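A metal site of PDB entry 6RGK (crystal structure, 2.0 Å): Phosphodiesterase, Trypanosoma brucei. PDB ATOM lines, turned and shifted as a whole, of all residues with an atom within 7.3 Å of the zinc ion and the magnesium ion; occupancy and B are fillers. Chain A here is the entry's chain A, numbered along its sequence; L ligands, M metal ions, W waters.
O of Ala 148 is in hydrogen-bond range of ND1 of His 151, at 2.7 Å.
The zinc ion is bound by water W6 (1.9 Å), NE2 of His 151 (2.0 Å), OD1 of Asp 264 (2.1 Å), OD2 of Asp 152 (2.1 Å), NE2 of His 115 (2.2 Å) and water W1 (2.3 Å). The zinc ion has six donor atoms within binding distance.
Water W6 lies within hydrogen-bond range of NE2 of His 111 (3.2 Å) and OD2 of Asp 264 (3.3 Å). Water W5 bridges the backbone carbonyl oxygen of His 151 and the side-chain hydroxyl of Thr 225. Water W2 lies within hydrogen-bond range of OE2 of Glu 184 (3.0 Å) and O of Thr 225 (3.0 Å).
Two residues have an atom within 4 Å of the magnesium ion: His 151 and Asp 152.
The magnesium ion is bound by water W1 (1.9 Å), water W5 (2.0 Å), water W3 (2.0 Å), water W4 (2.0 Å), the side-chain carboxylate of Asp 152 (2.0 Å) and water W2 (2.2 Å). The magnesium ion has six donor atoms within binding distance.
Of the 20 residues printed, 4 come within 4 Å of the zinc ion. Along chain A the residues within 4 Å of the zinc ion span positions 115 to 264. The nearest printed residue that does not touch the zinc ion is His 111 (4.3 Å).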
ATOM      1  N   TYR A 110     -15.938  17.027 -25.277  1.00  0.00           N
ATOM      2  CA  TYR A 110     -16.299  17.740 -24.011  1.00  0.00           C
ATOM      3  C   TYR A 110     -15.529  17.207 -22.813  1.00  0.00           C
ATOM      4  O   TYR A 110     -14.754  17.967 -22.218  1.00  0.00           O
ATOM      5  CB  TYR A 110     -17.790  17.666 -23.710  1.00  0.00           C
ATOM      6  CG  TYR A 110     -18.169  18.468 -22.487  1.00  0.00           C
ATOM      7  CD1 TYR A 110     -18.293  19.839 -22.564  1.00  0.00           C
ATOM      8  CD2 TYR A 110     -18.380  17.861 -21.263  1.00  0.00           C
ATOM      9  CE1 TYR A 110     -18.648  20.595 -21.452  1.00  0.00           C
ATOM     10  CE2 TYR A 110     -18.729  18.601 -20.133  1.00  0.00           C
ATOM     11  CZ  TYR A 110     -18.858  19.978 -20.237  1.00  0.00           C
ATOM     12  OH  TYR A 110     -19.173  20.732 -19.147  1.00  0.00           O
ATOM     13  N   HIS A 111     -15.700  15.927 -22.479  1.00  0.00           N
ATOM     14  CA  HIS A 111     -15.032  15.290 -21.322  1.00  0.00           C
ATOM     15  C   HIS A 111     -13.580  14.994 -21.671  1.00  0.00           C
ATOM     16  O   HIS A 111     -13.146  13.845 -21.518  1.00  0.00           O
ATOM     17  CB  HIS A 111     -15.791  14.056 -20.873  1.00  0.00           C
ATOM     18  CG  HIS A 111     -17.151  14.374 -20.351  1.00  0.00           C
ATOM     19  ND1 HIS A 111     -18.282  14.091 -21.046  1.00  0.00           N
ATOM     20  CD2 HIS A 111     -17.544  14.953 -19.198  1.00  0.00           C
ATOM     21  CE1 HIS A 111     -19.324  14.448 -20.343  1.00  0.00           C
ATOM     22  NE2 HIS A 111     -18.902  15.006 -19.216  1.00  0.00           N
ATOM     23  N   HIS A 115     -11.926  20.373 -20.192  1.00  0.00           N
ATOM     24  CA  HIS A 115     -13.073  20.354 -19.248  1.00  0.00           C
ATOM     25  C   HIS A 115     -12.576  20.342 -17.808  1.00  0.00           C
ATOM     26  O   HIS A 115     -13.067  21.149 -17.021  1.00  0.00           O
ATOM     27  CB  HIS A 115     -14.028  19.193 -19.527  1.00  0.00           C
ATOM     28  CG  HIS A 115     -15.006  18.948 -18.422  1.00  0.00           C
ATOM     29  ND1 HIS A 115     -15.944  19.893 -18.053  1.00  0.00           N
ATOM     30  CD2 HIS A 115     -15.182  17.901 -17.606  1.00  0.00           C
ATOM     31  CE1 HIS A 115     -16.674  19.415 -17.067  1.00  0.00           C
ATOM     32  NE2 HIS A 115     -16.247  18.193 -16.782  1.00  0.00           N
ATOM     33  N   VAL A 116     -11.628  19.475 -17.447  1.00  0.00           N
ATOM     34  CA  VAL A 116     -11.271  19.290 -16.007  1.00  0.00           C
ATOM     35  C   VAL A 116     -10.341  20.436 -15.565  1.00  0.00           C
ATOM     36  O   VAL A 116     -10.370  20.805 -14.356  1.00  0.00           O
ATOM     37  CB  VAL A 116     -10.698  17.881 -15.732  1.00  0.00           C
ATOM     38  CG1 VAL A 116     -11.583  16.786 -16.339  1.00  0.00           C
ATOM     39  CG2 VAL A 116      -9.268  17.687 -16.186  1.00  0.00           C
ATOM     40  N   VAL A 119     -12.874  23.021 -14.779  1.00  0.00           N
ATOM     41  CA  VAL A 119     -13.525  22.752 -13.458  1.00  0.00           C
ATOM     42  C   VAL A 119     -12.564  23.202 -12.341  1.00  0.00           C
ATOM     43  O   VAL A 119     -13.008  23.893 -11.419  1.00  0.00           O
ATOM     44  CB  VAL A 119     -13.986  21.290 -13.298  1.00  0.00           C
ATOM     45  CG1 VAL A 119     -14.482  21.006 -11.868  1.00  0.00           C
ATOM     46  CG2 VAL A 119     -15.055  20.947 -14.326  1.00  0.00           C
ATOM     47  N   ALA A 148     -10.559  18.217  -8.958  1.00  0.00           N
ATOM     48  CA  ALA A 148     -11.046  18.748 -10.251  1.00  0.00           C
ATOM     49  C   ALA A 148     -10.369  17.987 -11.400  1.00  0.00           C
ATOM     50  O   ALA A 148     -11.058  17.622 -12.369  1.00  0.00           O
ATOM     51  CB  ALA A 148     -10.759  20.216 -10.343  1.00  0.00           C
ATOM     52  N   HIS A 151     -11.466  14.051 -11.905  1.00  0.00           N
ATOM     53  CA  HIS A 151     -12.916  13.750 -11.723  1.00  0.00           C
ATOM     54  C   HIS A 151     -13.587  13.127 -12.975  1.00  0.00           C
ATOM     55  O   HIS A 151     -14.753  12.678 -12.862  1.00  0.00           O
ATOM     56  CB  HIS A 151     -13.666  14.999 -11.207  1.00  0.00           C
ATOM     57  CG  HIS A 151     -14.285  15.823 -12.293  1.00  0.00           C
ATOM     58  ND1 HIS A 151     -13.603  16.874 -12.903  1.00  0.00           N
ATOM     59  CD2 HIS A 151     -15.459  15.702 -12.935  1.00  0.00           C
ATOM     60  CE1 HIS A 151     -14.367  17.384 -13.835  1.00  0.00           C
ATOM     61  NE2 HIS A 151     -15.509  16.680 -13.896  1.00  0.00           N
ATOM     62  N   ASP A 152     -12.919  13.134 -14.131  1.00  0.00           N
ATOM     63  CA  ASP A 152     -13.460  12.501 -15.371  1.00  0.00           C
ATOM     64  C   ASP A 152     -12.389  11.631 -16.078  1.00  0.00           C
ATOM     65  O   ASP A 152     -12.581  11.373 -17.281  1.00  0.00           O
ATOM     66  CB  ASP A 152     -13.986  13.573 -16.328  1.00  0.00           C
ATOM     67  CG  ASP A 152     -15.393  14.050 -16.005  1.00  0.00           C
ATOM     68  OD1 ASP A 152     -16.212  13.221 -15.547  1.00  0.00           O
ATOM     69  OD2 ASP A 152     -15.660  15.239 -16.223  1.00  0.00           O
ATOM     70  N   LEU A 153     -11.353  11.167 -15.383  1.00  0.00           N
ATOM     71  CA  LEU A 153     -10.229  10.383 -16.006  1.00  0.00           C
ATOM     72  C   LEU A 153     -10.778   9.275 -16.912  1.00  0.00           C
ATOM     73  O   LEU A 153     -11.617   8.476 -16.459  1.00  0.00           O
ATOM     74  CB  LEU A 153      -9.340   9.757 -14.938  1.00  0.00           C
ATOM     75  CG  LEU A 153      -8.459  10.716 -14.155  1.00  0.00           C
ATOM     76  CD1 LEU A 153      -7.871  10.016 -12.947  1.00  0.00           C
ATOM     77  CD2 LEU A 153      -7.360  11.310 -15.018  1.00  0.00           C
ATOM     78  N   HIS A 155     -12.551   9.221 -19.641  1.00  0.00           N
ATOM     79  CA  HIS A 155     -13.957   9.395 -20.101  1.00  0.00           C
ATOM     80  C   HIS A 155     -13.966   9.211 -21.621  1.00  0.00           C
ATOM     81  O   HIS A 155     -13.108   9.798 -22.303  1.00  0.00           O
ATOM     82  CB  HIS A 155     -14.505  10.772 -19.673  1.00  0.00           C
ATOM     83  CG  HIS A 155     -15.991  10.862 -19.668  1.00  0.00           C
ATOM     84  ND1 HIS A 155     -16.748  10.672 -20.813  1.00  0.00           N
ATOM     85  CD2 HIS A 155     -16.872  11.129 -18.669  1.00  0.00           C
ATOM     86  CE1 HIS A 155     -18.033  10.798 -20.510  1.00  0.00           C
ATOM     87  NE2 HIS A 155     -18.132  11.069 -19.194  1.00  0.00           N
ATOM     88  N   LEU A 183     -18.984   5.211 -14.520  1.00  0.00           N
ATOM     89  CA  LEU A 183     -17.809   6.047 -14.899  1.00  0.00           C
ATOM     90  C   LEU A 183     -17.107   6.558 -13.642  1.00  0.00           C
ATOM     91  O   LEU A 183     -15.854   6.581 -13.625  1.00  0.00           O
ATOM     92  CB  LEU A 183     -18.262   7.218 -15.773  1.00  0.00           C
ATOM     93  CG  LEU A 183     -18.598   6.871 -17.221  1.00  0.00           C
ATOM     94  CD1 LEU A 183     -19.581   7.876 -17.817  1.00  0.00           C
ATOM     95  CD2 LEU A 183     -17.343   6.786 -18.053  1.00  0.00           C
ATOM     96  N   GLU A 184     -17.870   6.972 -12.630  1.00  0.00           N
ATOM     97  CA  GLU A 184     -17.313   7.697 -11.460  1.00  0.00           C
ATOM     98  C   GLU A 184     -16.400   6.759 -10.689  1.00  0.00           C
ATOM     99  O   GLU A 184     -15.300   7.193 -10.322  1.00  0.00           O
ATOM    100  CB  GLU A 184     -18.415   8.304 -10.594  1.00  0.00           C
ATOM    101  CG  GLU A 184     -19.196   9.391 -11.332  1.00  0.00           C
ATOM    102  CD  GLU A 184     -20.242   8.947 -12.337  1.00  0.00           C
ATOM    103  OE1 GLU A 184     -20.565   7.724 -12.397  1.00  0.00           O
ATOM    104  OE2 GLU A 184     -20.745   9.831 -13.061  1.00  0.00           O
ATOM    105  N   HIS A 187     -13.210   6.485 -12.690  1.00  0.00           N
ATOM    106  CA  HIS A 187     -12.345   7.695 -12.495  1.00  0.00           C
ATOM    107  C   HIS A 187     -11.561   7.491 -11.202  1.00  0.00           C
ATOM    108  O   HIS A 187     -10.339   7.670 -11.195  1.00  0.00           O
ATOM    109  CB  HIS A 187     -13.140   9.022 -12.498  1.00  0.00           C
ATOM    110  CG  HIS A 187     -14.099   9.215 -13.616  1.00  0.00           C
ATOM    111  ND1 HIS A 187     -13.786   8.911 -14.927  1.00  0.00           N
ATOM    112  CD2 HIS A 187     -15.373   9.656 -13.619  1.00  0.00           C
ATOM    113  CE1 HIS A 187     -14.817   9.165 -15.693  1.00  0.00           C
ATOM    114  NE2 HIS A 187     -15.814   9.634 -14.914  1.00  0.00           N
ATOM    115  N   VAL A 222     -15.861  12.821  -6.285  1.00  0.00           N
ATOM    116  CA  VAL A 222     -15.967  12.238  -7.651  1.00  0.00           C
ATOM    117  C   VAL A 222     -17.253  11.424  -7.754  1.00  0.00           C
ATOM    118  O   VAL A 222     -17.978  11.581  -8.760  1.00  0.00           O
ATOM    119  CB  VAL A 222     -14.734  11.375  -7.987  1.00  0.00           C
ATOM    120  CG1 VAL A 222     -14.892  10.715  -9.354  1.00  0.00           C
ATOM    121  CG2 VAL A 222     -13.461  12.177  -7.913  1.00  0.00           C
ATOM    122  N   THR A 225     -20.404  13.406  -8.343  1.00  0.00           N
ATOM    123  CA  THR A 225     -20.588  14.071  -9.675  1.00  0.00           C
ATOM    124  C   THR A 225     -21.558  13.284 -10.565  1.00  0.00           C
ATOM    125  O   THR A 225     -21.880  13.816 -11.675  1.00  0.00           O
ATOM    126  CB  THR A 225     -19.251  14.284 -10.403  1.00  0.00           C
ATOM    127  OG1 THR A 225     -18.608  13.054 -10.762  1.00  0.00           O
ATOM    128  CG2 THR A 225     -18.327  15.117  -9.545  1.00  0.00           C
ATOM    129  N   ASP A 226     -21.982  12.075 -10.170  1.00  0.00           N
ATOM    130  CA  ASP A 226     -22.991  11.293 -10.919  1.00  0.00           C
ATOM    131  C   ASP A 226     -24.329  12.018 -10.824  1.00  0.00           C
ATOM    132  O   ASP A 226     -24.887  12.070  -9.711  1.00  0.00           O
ATOM    133  CB  ASP A 226     -23.112   9.872 -10.376  1.00  0.00           C
ATOM    134  CG  ASP A 226     -24.120   8.973 -11.079  1.00  0.00           C
ATOM    135  OD1 ASP A 226     -24.973   9.492 -11.831  1.00  0.00           O
ATOM    136  OD2 ASP A 226     -24.042   7.764 -10.868  1.00  0.00           O
ATOM    137  N   LEU A 260     -17.565  20.680  -6.017  1.00  0.00           N
ATOM    138  CA  LEU A 260     -17.143  19.946  -7.232  1.00  0.00           C
ATOM    139  C   LEU A 260     -18.330  19.869  -8.193  1.00  0.00           C
ATOM    140  O   LEU A 260     -18.133  20.133  -9.346  1.00  0.00           O
ATOM    141  CB  LEU A 260     -16.630  18.548  -6.877  1.00  0.00           C
ATOM    142  CG  LEU A 260     -16.089  17.760  -8.060  1.00  0.00           C
ATOM    143  CD1 LEU A 260     -14.968  18.490  -8.734  1.00  0.00           C
ATOM    144  CD2 LEU A 260     -15.629  16.386  -7.646  1.00  0.00           C
ATOM    145  N   GLY A 263     -18.799  23.281  -9.973  1.00  0.00           N
ATOM    146  CA  GLY A 263     -17.834  23.474 -11.058  1.00  0.00           C
ATOM    147  C   GLY A 263     -18.236  22.647 -12.265  1.00  0.00           C
ATOM    148  O   GLY A 263     -18.083  23.133 -13.396  1.00  0.00           O
ATOM    149  N   ASP A 264     -18.698  21.432 -12.011  1.00  0.00           N
ATOM    150  CA  ASP A 264     -19.033  20.446 -13.068  1.00  0.00           C
ATOM    151  C   ASP A 264     -20.230  20.941 -13.889  1.00  0.00           C
ATOM    152  O   ASP A 264     -20.275  20.582 -15.038  1.00  0.00           O
ATOM    153  CB  ASP A 264     -19.300  19.056 -12.476  1.00  0.00           C
ATOM    154  CG  ASP A 264     -18.994  17.902 -13.428  1.00  0.00           C
ATOM    155  OD1 ASP A 264     -18.134  18.095 -14.318  1.00  0.00           O
ATOM    156  OD2 ASP A 264     -19.622  16.821 -13.254  1.00  0.00           O
ATOM    157  N   ILE A 265     -21.170  21.713 -13.317  1.00  0.00           N
ATOM    158  CA  ILE A 265     -22.272  22.321 -14.137  1.00  0.00           C
ATOM    159  C   ILE A 265     -22.144  23.852 -14.215  1.00  0.00           C
ATOM    160  O   ILE A 265     -23.175  24.521 -14.349  1.00  0.00           O
ATOM    161  CB  ILE A 265     -23.643  21.865 -13.584  1.00  0.00           C
ATOM    162  CG1 ILE A 265     -23.892  22.321 -12.154  1.00  0.00           C
ATOM    163  CG2 ILE A 265     -23.775  20.355 -13.700  1.00  0.00           C
ATOM    164  CD1 ILE A 265     -25.344  22.201 -11.731  1.00  0.00           C
HETATM  165  C1  LIG L   1     -23.509  17.079 -17.647  1.00  0.00           C
HETATM  166  C2  LIG L   1     -23.494  17.695 -16.257  1.00  0.00           C
HETATM  167  C3  LIG L   1     -22.626  16.964 -15.298  1.00  0.00           C
HETATM  168  C4  LIG L   1     -22.317  15.692 -15.424  1.00  0.00           C
HETATM  169  C5  LIG L   1     -22.452  14.942 -16.697  1.00  0.00           C
HETATM  170  C6  LIG L   1     -24.912  15.095 -17.217  1.00  0.00           C
HETATM  171  C7  LIG L   1     -28.357  21.187 -23.529  1.00  0.00           C
HETATM  172  C8  LIG L   1     -27.323  21.001 -22.578  1.00  0.00           C
HETATM  173  C9  LIG L   1     -32.360  19.317 -19.928  1.00  0.00           C
HETATM  174  C10 LIG L   1     -26.482  20.759 -21.753  1.00  0.00           C
HETATM  175  C11 LIG L   1     -25.516  20.419 -20.759  1.00  0.00           C
HETATM  176  C12 LIG L   1     -24.464  21.318 -20.454  1.00  0.00           C
HETATM  177  C13 LIG L   1     -31.189  19.994 -20.601  1.00  0.00           C
HETATM  178  C14 LIG L   1     -23.230  23.210 -21.250  1.00  0.00           C
HETATM  179  C15 LIG L   1     -31.083  19.648 -22.083  1.00  0.00           C
HETATM  180  C16 LIG L   1     -29.665  19.370 -22.525  1.00  0.00           C
HETATM  181  C17 LIG L   1     -23.531  20.975 -19.491  1.00  0.00           C
HETATM  182  C18 LIG L   1     -24.639  18.870 -19.127  1.00  0.00           C
HETATM  183  C19 LIG L   1     -27.333  15.495 -17.252  1.00  0.00           C
HETATM  184  C20 LIG L   1     -23.622  19.764 -18.832  1.00  0.00           C
HETATM  185  C21 LIG L   1     -25.592  19.200 -20.089  1.00  0.00           C
HETATM  186  C22 LIG L   1     -24.715  17.567 -18.402  1.00  0.00           C
HETATM  187  C23 LIG L   1     -27.985  16.601 -16.427  1.00  0.00           C
HETATM  188  C24 LIG L   1     -29.372  16.264 -15.895  1.00  0.00           C
HETATM  189  C25 LIG L   1     -30.499  16.627 -16.826  1.00  0.00           C
HETATM  190  C26 LIG L   1     -30.599  15.747 -18.055  1.00  0.00           C
HETATM  191  C27 LIG L   1     -29.602  14.616 -18.086  1.00  0.00           C
HETATM  192  C28 LIG L   1     -28.182  15.044 -18.441  1.00  0.00           C
HETATM  193  C29 LIG L   1     -23.538  15.546 -17.602  1.00  0.00           C
HETATM  194  N1  LIG L   1     -29.249  20.195 -23.655  1.00  0.00           N
HETATM  195  N2  LIG L   1     -25.833  16.929 -18.466  1.00  0.00           N
HETATM  196  N3  LIG L   1     -25.954  15.849 -17.661  1.00  0.00           N
HETATM  197  O1  LIG L   1     -28.400  22.232 -24.173  1.00  0.00           O
HETATM  198  O2  LIG L   1     -24.458  22.493 -21.151  1.00  0.00           O
HETATM  199  O3  LIG L   1     -25.100  14.096 -16.543  1.00  0.00           O
HETATM  200 ZN    ZN M   1     -16.905  16.706 -15.326  1.00  0.00          ZN
HETATM  201 MG    MG M   2     -18.137  13.051 -14.904  1.00  0.00          MG
HETATM  202  O   HOH W   1     -18.081  14.922 -14.457  1.00  0.00           O
HETATM  203  O   HOH W   2     -19.975  12.663 -13.714  1.00  0.00           O
HETATM  204  O   HOH W   3     -19.186  13.476 -16.570  1.00  0.00           O
HETATM  205  O   HOH W   4     -18.228  11.079 -15.375  1.00  0.00           O
HETATM  206  O   HOH W   5     -17.420  12.532 -13.162  1.00  0.00           O
HETATM  207  O   HOH W   6     -18.542  16.311 -16.288  1.00  0.00           O
